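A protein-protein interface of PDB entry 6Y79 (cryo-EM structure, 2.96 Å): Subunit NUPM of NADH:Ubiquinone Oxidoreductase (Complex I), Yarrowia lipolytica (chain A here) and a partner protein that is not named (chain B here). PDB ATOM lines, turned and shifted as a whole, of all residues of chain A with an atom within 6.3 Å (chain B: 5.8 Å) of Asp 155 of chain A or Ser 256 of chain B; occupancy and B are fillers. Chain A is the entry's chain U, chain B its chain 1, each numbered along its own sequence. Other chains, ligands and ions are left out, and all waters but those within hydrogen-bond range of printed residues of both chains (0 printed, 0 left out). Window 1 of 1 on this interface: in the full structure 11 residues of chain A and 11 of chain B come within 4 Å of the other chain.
Asn 104 of chain A touches none of the printed residues of chain B. Of the printed residues of chain B, Asp 155 of chain A touches Ser 256 and Asn 260. Of the printed residues of chain B, Asp 156 of chain A touches Tyr 266 (3.2 Å). Of the printed residues of chain B, Phe 157 of chain A touches Phe 259 and Asn 260. Of the printed residues of chain A, Ser 256 of chain B touches Ala 153 and Asp 155. Printed residues of chain A within 4 Å of Asn 260 of chain B: Asp 155, Phe 157 and Val 160. The nearest residue of chain B that does not touch Asp 155 of chain A is Tyr 266 of chain B (4.9 Å). The nearest residue of chain A that does not touch Ser 256 of chain B is Val 154 of chain A (4.3 Å). The nearest printed residue of chain A that does not touch Asn 254 of chain B is Lys 151 of chain A (4.5 Å).
The backbone carbonyl oxygen of Asp 156 of chain A lies within hydrogen-bond range of the side-chain hydroxyl of Ser 159 of chain A (3.2 Å). The side-chain amide nitrogen of Asn 260 of chain B sits at hydrogen-bond distance from the backbone carbonyl oxygen of Ser 256 of chain B (3.1 Å).
Of the 12 printed residues of chain A, 7 touch a printed residue of chain B. Hydrophobic or aromatic side chains of chain A within 4 Å of the printed part of chain B: Val 154, Phe 157 and Val 160. Of the 9 printed residues of chain B, 6 touch a printed residue of chain A. Hydrophobic or aromatic side chains of chain B that line the printed part of chain A: Tyr 255, Phe 259 and Tyr 266. Among the printed residues, 11 pairs touch across the chains. Among the printed residues, no Asp or Glu carboxylate lies within 4 Å of a Lys or Arg side-chain nitrogen of the other chain.
The backbone carbonyl oxygen (O) of Ala 153 of chain A lies close to the backbone carbonyl oxygen (O) of Asn 254 of chain B. The backbone NH (N) of Asp 155 of chain A is in hydrogen-bond range of the side-chain hydroxyl (OG) of Ser 256 of chain B (3.4 Å).
O of Pro 152 of chain A touches OD1 of Asn 254 of chain B, 3.8 Å away. O of Ala 153 of chain A touches CB of Ser 256 of chain B, 3.97 Å away. Val 154 of chain A touches Tyr 255 of chain B (CG2 to CE1, 3.8 Å). CD2 of Phe 259 of chain B touches CG1 of Val 154 of chain A, at 3.6 Å. O of Asp 155 of chain A touches OD1 of Asn 260 of chain B, at 3.8 Å. OD1 of Asp 156 of chain A touches CE2 of Tyr 266 of chain B, at 3.2 Å. Phe 157 of chain A touches Phe 259 of chain B (CE1 to O, 3.2 Å). Asn 260 of chain B touches Phe 157 of chain A (OD1 to CD1, 3.2 Å). Asn 260 of chain B touches Val 160 of chain A.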
ATOM      1  N   ASN A 104      20.160 -27.398   1.405  1.00  0.00           N
ATOM      2  CA  ASN A 104      19.744 -28.422   2.376  1.00  0.00           C
ATOM      3  C   ASN A 104      19.601 -29.812   1.757  1.00  0.00           C
ATOM      4  O   ASN A 104      18.690 -30.548   2.119  1.00  0.00           O
ATOM      5  CB  ASN A 104      18.438 -28.039   3.086  1.00  0.00           C
ATOM      6  CG  ASN A 104      18.585 -26.841   3.980  1.00  0.00           C
ATOM      7  OD1 ASN A 104      19.566 -26.705   4.711  1.00  0.00           O
ATOM      8  ND2 ASN A 104      17.597 -25.960   3.937  1.00  0.00           N
ATOM      9  N   GLY A 110      13.715 -29.652   5.642  1.00  0.00           N
ATOM     10  CA  GLY A 110      14.171 -28.303   5.871  1.00  0.00           C
ATOM     11  C   GLY A 110      13.435 -27.213   5.129  1.00  0.00           C
ATOM     12  O   GLY A 110      13.955 -26.100   5.030  1.00  0.00           O
ATOM     13  N   LYS A 113       8.146 -24.233   5.838  1.00  0.00           N
ATOM     14  CA  LYS A 113       7.391 -22.989   5.769  1.00  0.00           C
ATOM     15  C   LYS A 113       7.113 -22.563   4.335  1.00  0.00           C
ATOM     16  O   LYS A 113       6.164 -21.814   4.094  1.00  0.00           O
ATOM     17  CB  LYS A 113       8.128 -21.889   6.531  1.00  0.00           C
ATOM     18  CG  LYS A 113       8.126 -22.125   8.022  1.00  0.00           C
ATOM     19  CD  LYS A 113       8.898 -21.066   8.773  1.00  0.00           C
ATOM     20  CE  LYS A 113       8.895 -21.379  10.258  1.00  0.00           C
ATOM     21  NZ  LYS A 113       9.626 -20.364  11.056  1.00  0.00           N
ATOM     22  N   LYS A 151      14.512 -29.940  12.836  1.00  0.00           N
ATOM     23  CA  LYS A 151      14.551 -28.610  12.278  1.00  0.00           C
ATOM     24  C   LYS A 151      15.786 -28.465  11.403  1.00  0.00           C
ATOM     25  O   LYS A 151      16.792 -29.139  11.633  1.00  0.00           O
ATOM     26  CB  LYS A 151      14.588 -27.569  13.396  1.00  0.00           C
ATOM     27  CG  LYS A 151      13.400 -27.637  14.325  1.00  0.00           C
ATOM     28  CD  LYS A 151      13.479 -26.571  15.390  1.00  0.00           C
ATOM     29  CE  LYS A 151      12.226 -26.563  16.239  1.00  0.00           C
ATOM     30  NZ  LYS A 151      12.297 -25.531  17.310  1.00  0.00           N
ATOM     31  N   PRO A 152      15.757 -27.631  10.374  1.00  0.00           N
ATOM     32  CA  PRO A 152      16.956 -27.425   9.562  1.00  0.00           C
ATOM     33  C   PRO A 152      17.955 -26.515  10.261  1.00  0.00           C
ATOM     34  O   PRO A 152      17.712 -25.982  11.343  1.00  0.00           O
ATOM     35  CB  PRO A 152      16.417 -26.781   8.289  1.00  0.00           C
ATOM     36  CG  PRO A 152      15.162 -26.168   8.687  1.00  0.00           C
ATOM     37  CD  PRO A 152      14.573 -27.019   9.755  1.00  0.00           C
ATOM     38  N   ALA A 153      19.108 -26.364   9.609  1.00  0.00           N
ATOM     39  CA  ALA A 153      20.178 -25.544  10.160  1.00  0.00           C
ATOM     40  C   ALA A 153      19.799 -24.074  10.153  1.00  0.00           C
ATOM     41  O   ALA A 153      19.775 -23.424  11.203  1.00  0.00           O
ATOM     42  CB  ALA A 153      21.463 -25.768   9.369  1.00  0.00           C
ATOM     43  N   VAL A 154      19.518 -23.526   8.972  1.00  0.00           N
ATOM     44  CA  VAL A 154      19.065 -22.149   8.808  1.00  0.00           C
ATOM     45  C   VAL A 154      17.830 -22.166   7.919  1.00  0.00           C
ATOM     46  O   VAL A 154      17.874 -22.715   6.811  1.00  0.00           O
ATOM     47  CB  VAL A 154      20.142 -21.240   8.189  1.00  0.00           C
ATOM     48  CG1 VAL A 154      19.674 -19.808   8.215  1.00  0.00           C
ATOM     49  CG2 VAL A 154      21.477 -21.361   8.902  1.00  0.00           C
ATOM     50  N   ASP A 155      16.733 -21.581   8.403  1.00  0.00           N
ATOM     51  CA  ASP A 155      15.570 -21.363   7.557  1.00  0.00           C
ATOM     52  C   ASP A 155      15.874 -20.316   6.501  1.00  0.00           C
ATOM     53  O   ASP A 155      16.527 -19.310   6.781  1.00  0.00           O
ATOM     54  CB  ASP A 155      14.379 -20.920   8.400  1.00  0.00           C
ATOM     55  CG  ASP A 155      13.973 -21.964   9.413  1.00  0.00           C
ATOM     56  OD1 ASP A 155      14.182 -23.147   9.106  1.00  0.00           O
ATOM     57  OD2 ASP A 155      13.445 -21.616  10.487  1.00  0.00           O
ATOM     58  N   ASP A 156      15.398 -20.559   5.283  1.00  0.00           N
ATOM     59  CA  ASP A 156      15.610 -19.629   4.188  1.00  0.00           C
ATOM     60  C   ASP A 156      14.848 -18.337   4.455  1.00  0.00           C
ATOM     61  O   ASP A 156      13.765 -18.334   5.040  1.00  0.00           O
ATOM     62  CB  ASP A 156      15.169 -20.251   2.857  1.00  0.00           C
ATOM     63  CG  ASP A 156      15.590 -19.429   1.630  1.00  0.00           C
ATOM     64  OD1 ASP A 156      16.178 -18.335   1.763  1.00  0.00           O
ATOM     65  OD2 ASP A 156      15.335 -19.902   0.508  1.00  0.00           O
ATOM     66  N   PHE A 157      15.441 -17.232   4.006  1.00  0.00           N
ATOM     67  CA  PHE A 157      14.960 -15.916   4.402  1.00  0.00           C
ATOM     68  C   PHE A 157      13.702 -15.525   3.641  1.00  0.00           C
ATOM     69  O   PHE A 157      12.769 -14.958   4.227  1.00  0.00           O
ATOM     70  CB  PHE A 157      16.065 -14.897   4.182  1.00  0.00           C
ATOM     71  CG  PHE A 157      17.297 -15.164   4.985  1.00  0.00           C
ATOM     72  CD1 PHE A 157      17.375 -14.740   6.293  1.00  0.00           C
ATOM     73  CD2 PHE A 157      18.377 -15.836   4.435  1.00  0.00           C
ATOM     74  CE1 PHE A 157      18.500 -14.983   7.043  1.00  0.00           C
ATOM     75  CE2 PHE A 157      19.509 -16.080   5.187  1.00  0.00           C
ATOM     76  CZ  PHE A 157      19.568 -15.652   6.491  1.00  0.00           C
ATOM     77  N   SER A 159      11.417 -17.464   2.392  1.00  0.00           N
ATOM     78  CA  SER A 159      10.251 -18.238   2.780  1.00  0.00           C
ATOM     79  C   SER A 159       9.757 -17.884   4.177  1.00  0.00           C
ATOM     80  O   SER A 159       8.550 -17.928   4.414  1.00  0.00           O
ATOM     81  CB  SER A 159      10.550 -19.732   2.676  1.00  0.00           C
ATOM     82  OG  SER A 159      11.538 -20.124   3.604  1.00  0.00           O
ATOM     83  N   VAL A 160      10.636 -17.491   5.102  1.00  0.00           N
ATOM     84  CA  VAL A 160      10.140 -17.058   6.408  1.00  0.00           C
ATOM     85  C   VAL A 160       9.522 -15.665   6.306  1.00  0.00           C
ATOM     86  O   VAL A 160       8.532 -15.361   6.987  1.00  0.00           O
ATOM     87  CB  VAL A 160      11.247 -17.152   7.484  1.00  0.00           C
ATOM     88  CG1 VAL A 160      12.405 -16.210   7.223  1.00  0.00           C
ATOM     89  CG2 VAL A 160      10.676 -16.916   8.874  1.00  0.00           C
ATOM     90  N   ASN B 254      21.016 -23.470  17.487  1.00  0.00           N
ATOM     91  CA  ASN B 254      20.174 -23.408  16.299  1.00  0.00           C
ATOM     92  C   ASN B 254      20.670 -22.359  15.304  1.00  0.00           C
ATOM     93  O   ASN B 254      20.800 -22.652  14.111  1.00  0.00           O
ATOM     94  CB  ASN B 254      18.724 -23.135  16.697  1.00  0.00           C
ATOM     95  CG  ASN B 254      17.741 -23.521  15.609  1.00  0.00           C
ATOM     96  OD1 ASN B 254      18.124 -24.078  14.581  1.00  0.00           O
ATOM     97  ND2 ASN B 254      16.467 -23.224  15.829  1.00  0.00           N
ATOM     98  N   TYR B 255      20.941 -21.140  15.792  1.00  0.00           N
ATOM     99  CA  TYR B 255      21.391 -19.955  15.027  1.00  0.00           C
ATOM    100  C   TYR B 255      20.565 -19.670  13.768  1.00  0.00           C
ATOM    101  O   TYR B 255      21.064 -19.105  12.797  1.00  0.00           O
ATOM    102  CB  TYR B 255      22.896 -20.000  14.695  1.00  0.00           C
ATOM    103  CG  TYR B 255      23.441 -21.120  13.825  1.00  0.00           C
ATOM    104  CD1 TYR B 255      23.490 -21.003  12.439  1.00  0.00           C
ATOM    105  CD2 TYR B 255      23.974 -22.264  14.396  1.00  0.00           C
ATOM    106  CE1 TYR B 255      24.003 -22.008  11.651  1.00  0.00           C
ATOM    107  CE2 TYR B 255      24.488 -23.279  13.615  1.00  0.00           C
ATOM    108  CZ  TYR B 255      24.502 -23.141  12.244  1.00  0.00           C
ATOM    109  OH  TYR B 255      25.017 -24.150  11.466  1.00  0.00           O
ATOM    110  N   SER B 256      19.279 -19.999  13.784  1.00  0.00           N
ATOM    111  CA  SER B 256      18.411 -19.573  12.698  1.00  0.00           C
ATOM    112  C   SER B 256      17.808 -18.203  12.960  1.00  0.00           C
ATOM    113  O   SER B 256      17.667 -17.402  12.032  1.00  0.00           O
ATOM    114  CB  SER B 256      17.298 -20.594  12.480  1.00  0.00           C
ATOM    115  OG  SER B 256      16.385 -20.141  11.499  1.00  0.00           O
ATOM    116  N   TYR B 257      17.454 -17.923  14.217  1.00  0.00           N
ATOM    117  CA  TYR B 257      16.836 -16.651  14.575  1.00  0.00           C
ATOM    118  C   TYR B 257      17.830 -15.503  14.464  1.00  0.00           C
ATOM    119  O   TYR B 257      17.474 -14.399  14.025  1.00  0.00           O
ATOM    120  CB  TYR B 257      16.269 -16.756  15.989  1.00  0.00           C
ATOM    121  CG  TYR B 257      15.560 -15.525  16.497  1.00  0.00           C
ATOM    122  CD1 TYR B 257      14.324 -15.153  15.985  1.00  0.00           C
ATOM    123  CD2 TYR B 257      16.115 -14.746  17.511  1.00  0.00           C
ATOM    124  CE1 TYR B 257      13.667 -14.030  16.457  1.00  0.00           C
ATOM    125  CE2 TYR B 257      15.466 -13.625  17.988  1.00  0.00           C
ATOM    126  CZ  TYR B 257      14.241 -13.272  17.458  1.00  0.00           C
ATOM    127  OH  TYR B 257      13.588 -12.156  17.926  1.00  0.00           O
ATOM    128  N   LEU B 258      19.085 -15.754  14.849  1.00  0.00           N
ATOM    129  CA  LEU B 258      20.141 -14.758  14.716  1.00  0.00           C
ATOM    130  C   LEU B 258      20.397 -14.408  13.259  1.00  0.00           C
ATOM    131  O   LEU B 258      20.669 -13.245  12.938  1.00  0.00           O
ATOM    132  CB  LEU B 258      21.418 -15.279  15.371  1.00  0.00           C
ATOM    133  CG  LEU B 258      22.646 -14.376  15.411  1.00  0.00           C
ATOM    134  CD1 LEU B 258      22.383 -13.163  16.276  1.00  0.00           C
ATOM    135  CD2 LEU B 258      23.836 -15.152  15.924  1.00  0.00           C
ATOM    136  N   PHE B 259      20.266 -15.383  12.361  1.00  0.00           N
ATOM    137  CA  PHE B 259      20.497 -15.112  10.947  1.00  0.00           C
ATOM    138  C   PHE B 259      19.339 -14.332  10.344  1.00  0.00           C
ATOM    139  O   PHE B 259      19.553 -13.399   9.565  1.00  0.00           O
ATOM    140  CB  PHE B 259      20.710 -16.411  10.175  1.00  0.00           C
ATOM    141  CG  PHE B 259      22.094 -16.985  10.296  1.00  0.00           C
ATOM    142  CD1 PHE B 259      22.978 -16.562  11.273  1.00  0.00           C
ATOM    143  CD2 PHE B 259      22.521 -17.939   9.397  1.00  0.00           C
ATOM    144  CE1 PHE B 259      24.238 -17.103  11.369  1.00  0.00           C
ATOM    145  CE2 PHE B 259      23.788 -18.478   9.483  1.00  0.00           C
ATOM    146  CZ  PHE B 259      24.647 -18.052  10.470  1.00  0.00           C
ATOM    147  N   ASN B 260      18.107 -14.683  10.718  1.00  0.00           N
ATOM    148  CA  ASN B 260      16.935 -13.937  10.279  1.00  0.00           C
ATOM    149  C   ASN B 260      16.886 -12.529  10.860  1.00  0.00           C
ATOM    150  O   ASN B 260      16.158 -11.683  10.334  1.00  0.00           O
ATOM    151  CB  ASN B 260      15.662 -14.692  10.651  1.00  0.00           C
ATOM    152  CG  ASN B 260      15.515 -15.997   9.895  1.00  0.00           C
ATOM    153  OD1 ASN B 260      15.865 -16.091   8.723  1.00  0.00           O
ATOM    154  ND2 ASN B 260      14.983 -17.010  10.564  1.00  0.00           N
ATOM    155  N   ILE B 261      17.621 -12.262  11.940  1.00  0.00           N
ATOM    156  CA  ILE B 261      17.879 -10.876  12.316  1.00  0.00           C
ATOM    157  C   ILE B 261      18.922 -10.260  11.392  1.00  0.00           C
ATOM    158  O   ILE B 261      18.703  -9.192  10.812  1.00  0.00           O
ATOM    159  CB  ILE B 261      18.312 -10.785  13.788  1.00  0.00           C
ATOM    160  CG1 ILE B 261      17.155 -11.160  14.707  1.00  0.00           C
ATOM    161  CG2 ILE B 261      18.807  -9.385  14.114  1.00  0.00           C
ATOM    162  CD1 ILE B 261      17.570 -11.282  16.138  1.00  0.00           C
ATOM    163  N   TYR B 266      21.234 -15.105   0.793  1.00  0.00           N
ATOM    164  CA  TYR B 266      22.489 -15.834   0.643  1.00  0.00           C
ATOM    165  C   TYR B 266      23.529 -14.998  -0.089  1.00  0.00           C
ATOM    166  O   TYR B 266      23.335 -14.624  -1.250  1.00  0.00           O
ATOM    167  CB  TYR B 266      22.235 -17.131  -0.120  1.00  0.00           C
ATOM    168  CG  TYR B 266      21.325 -18.072   0.608  1.00  0.00           C
ATOM    169  CD1 TYR B 266      21.806 -18.856   1.641  1.00  0.00           C
ATOM    170  CD2 TYR B 266      19.985 -18.167   0.276  1.00  0.00           C
ATOM    171  CE1 TYR B 266      20.978 -19.717   2.324  1.00  0.00           C
ATOM    172  CE2 TYR B 266      19.150 -19.029   0.954  1.00  0.00           C
ATOM    173  CZ  TYR B 266      19.653 -19.798   1.977  1.00  0.00           C
ATOM    174  OH  TYR B 266      18.826 -20.656   2.654  1.00  0.00           O
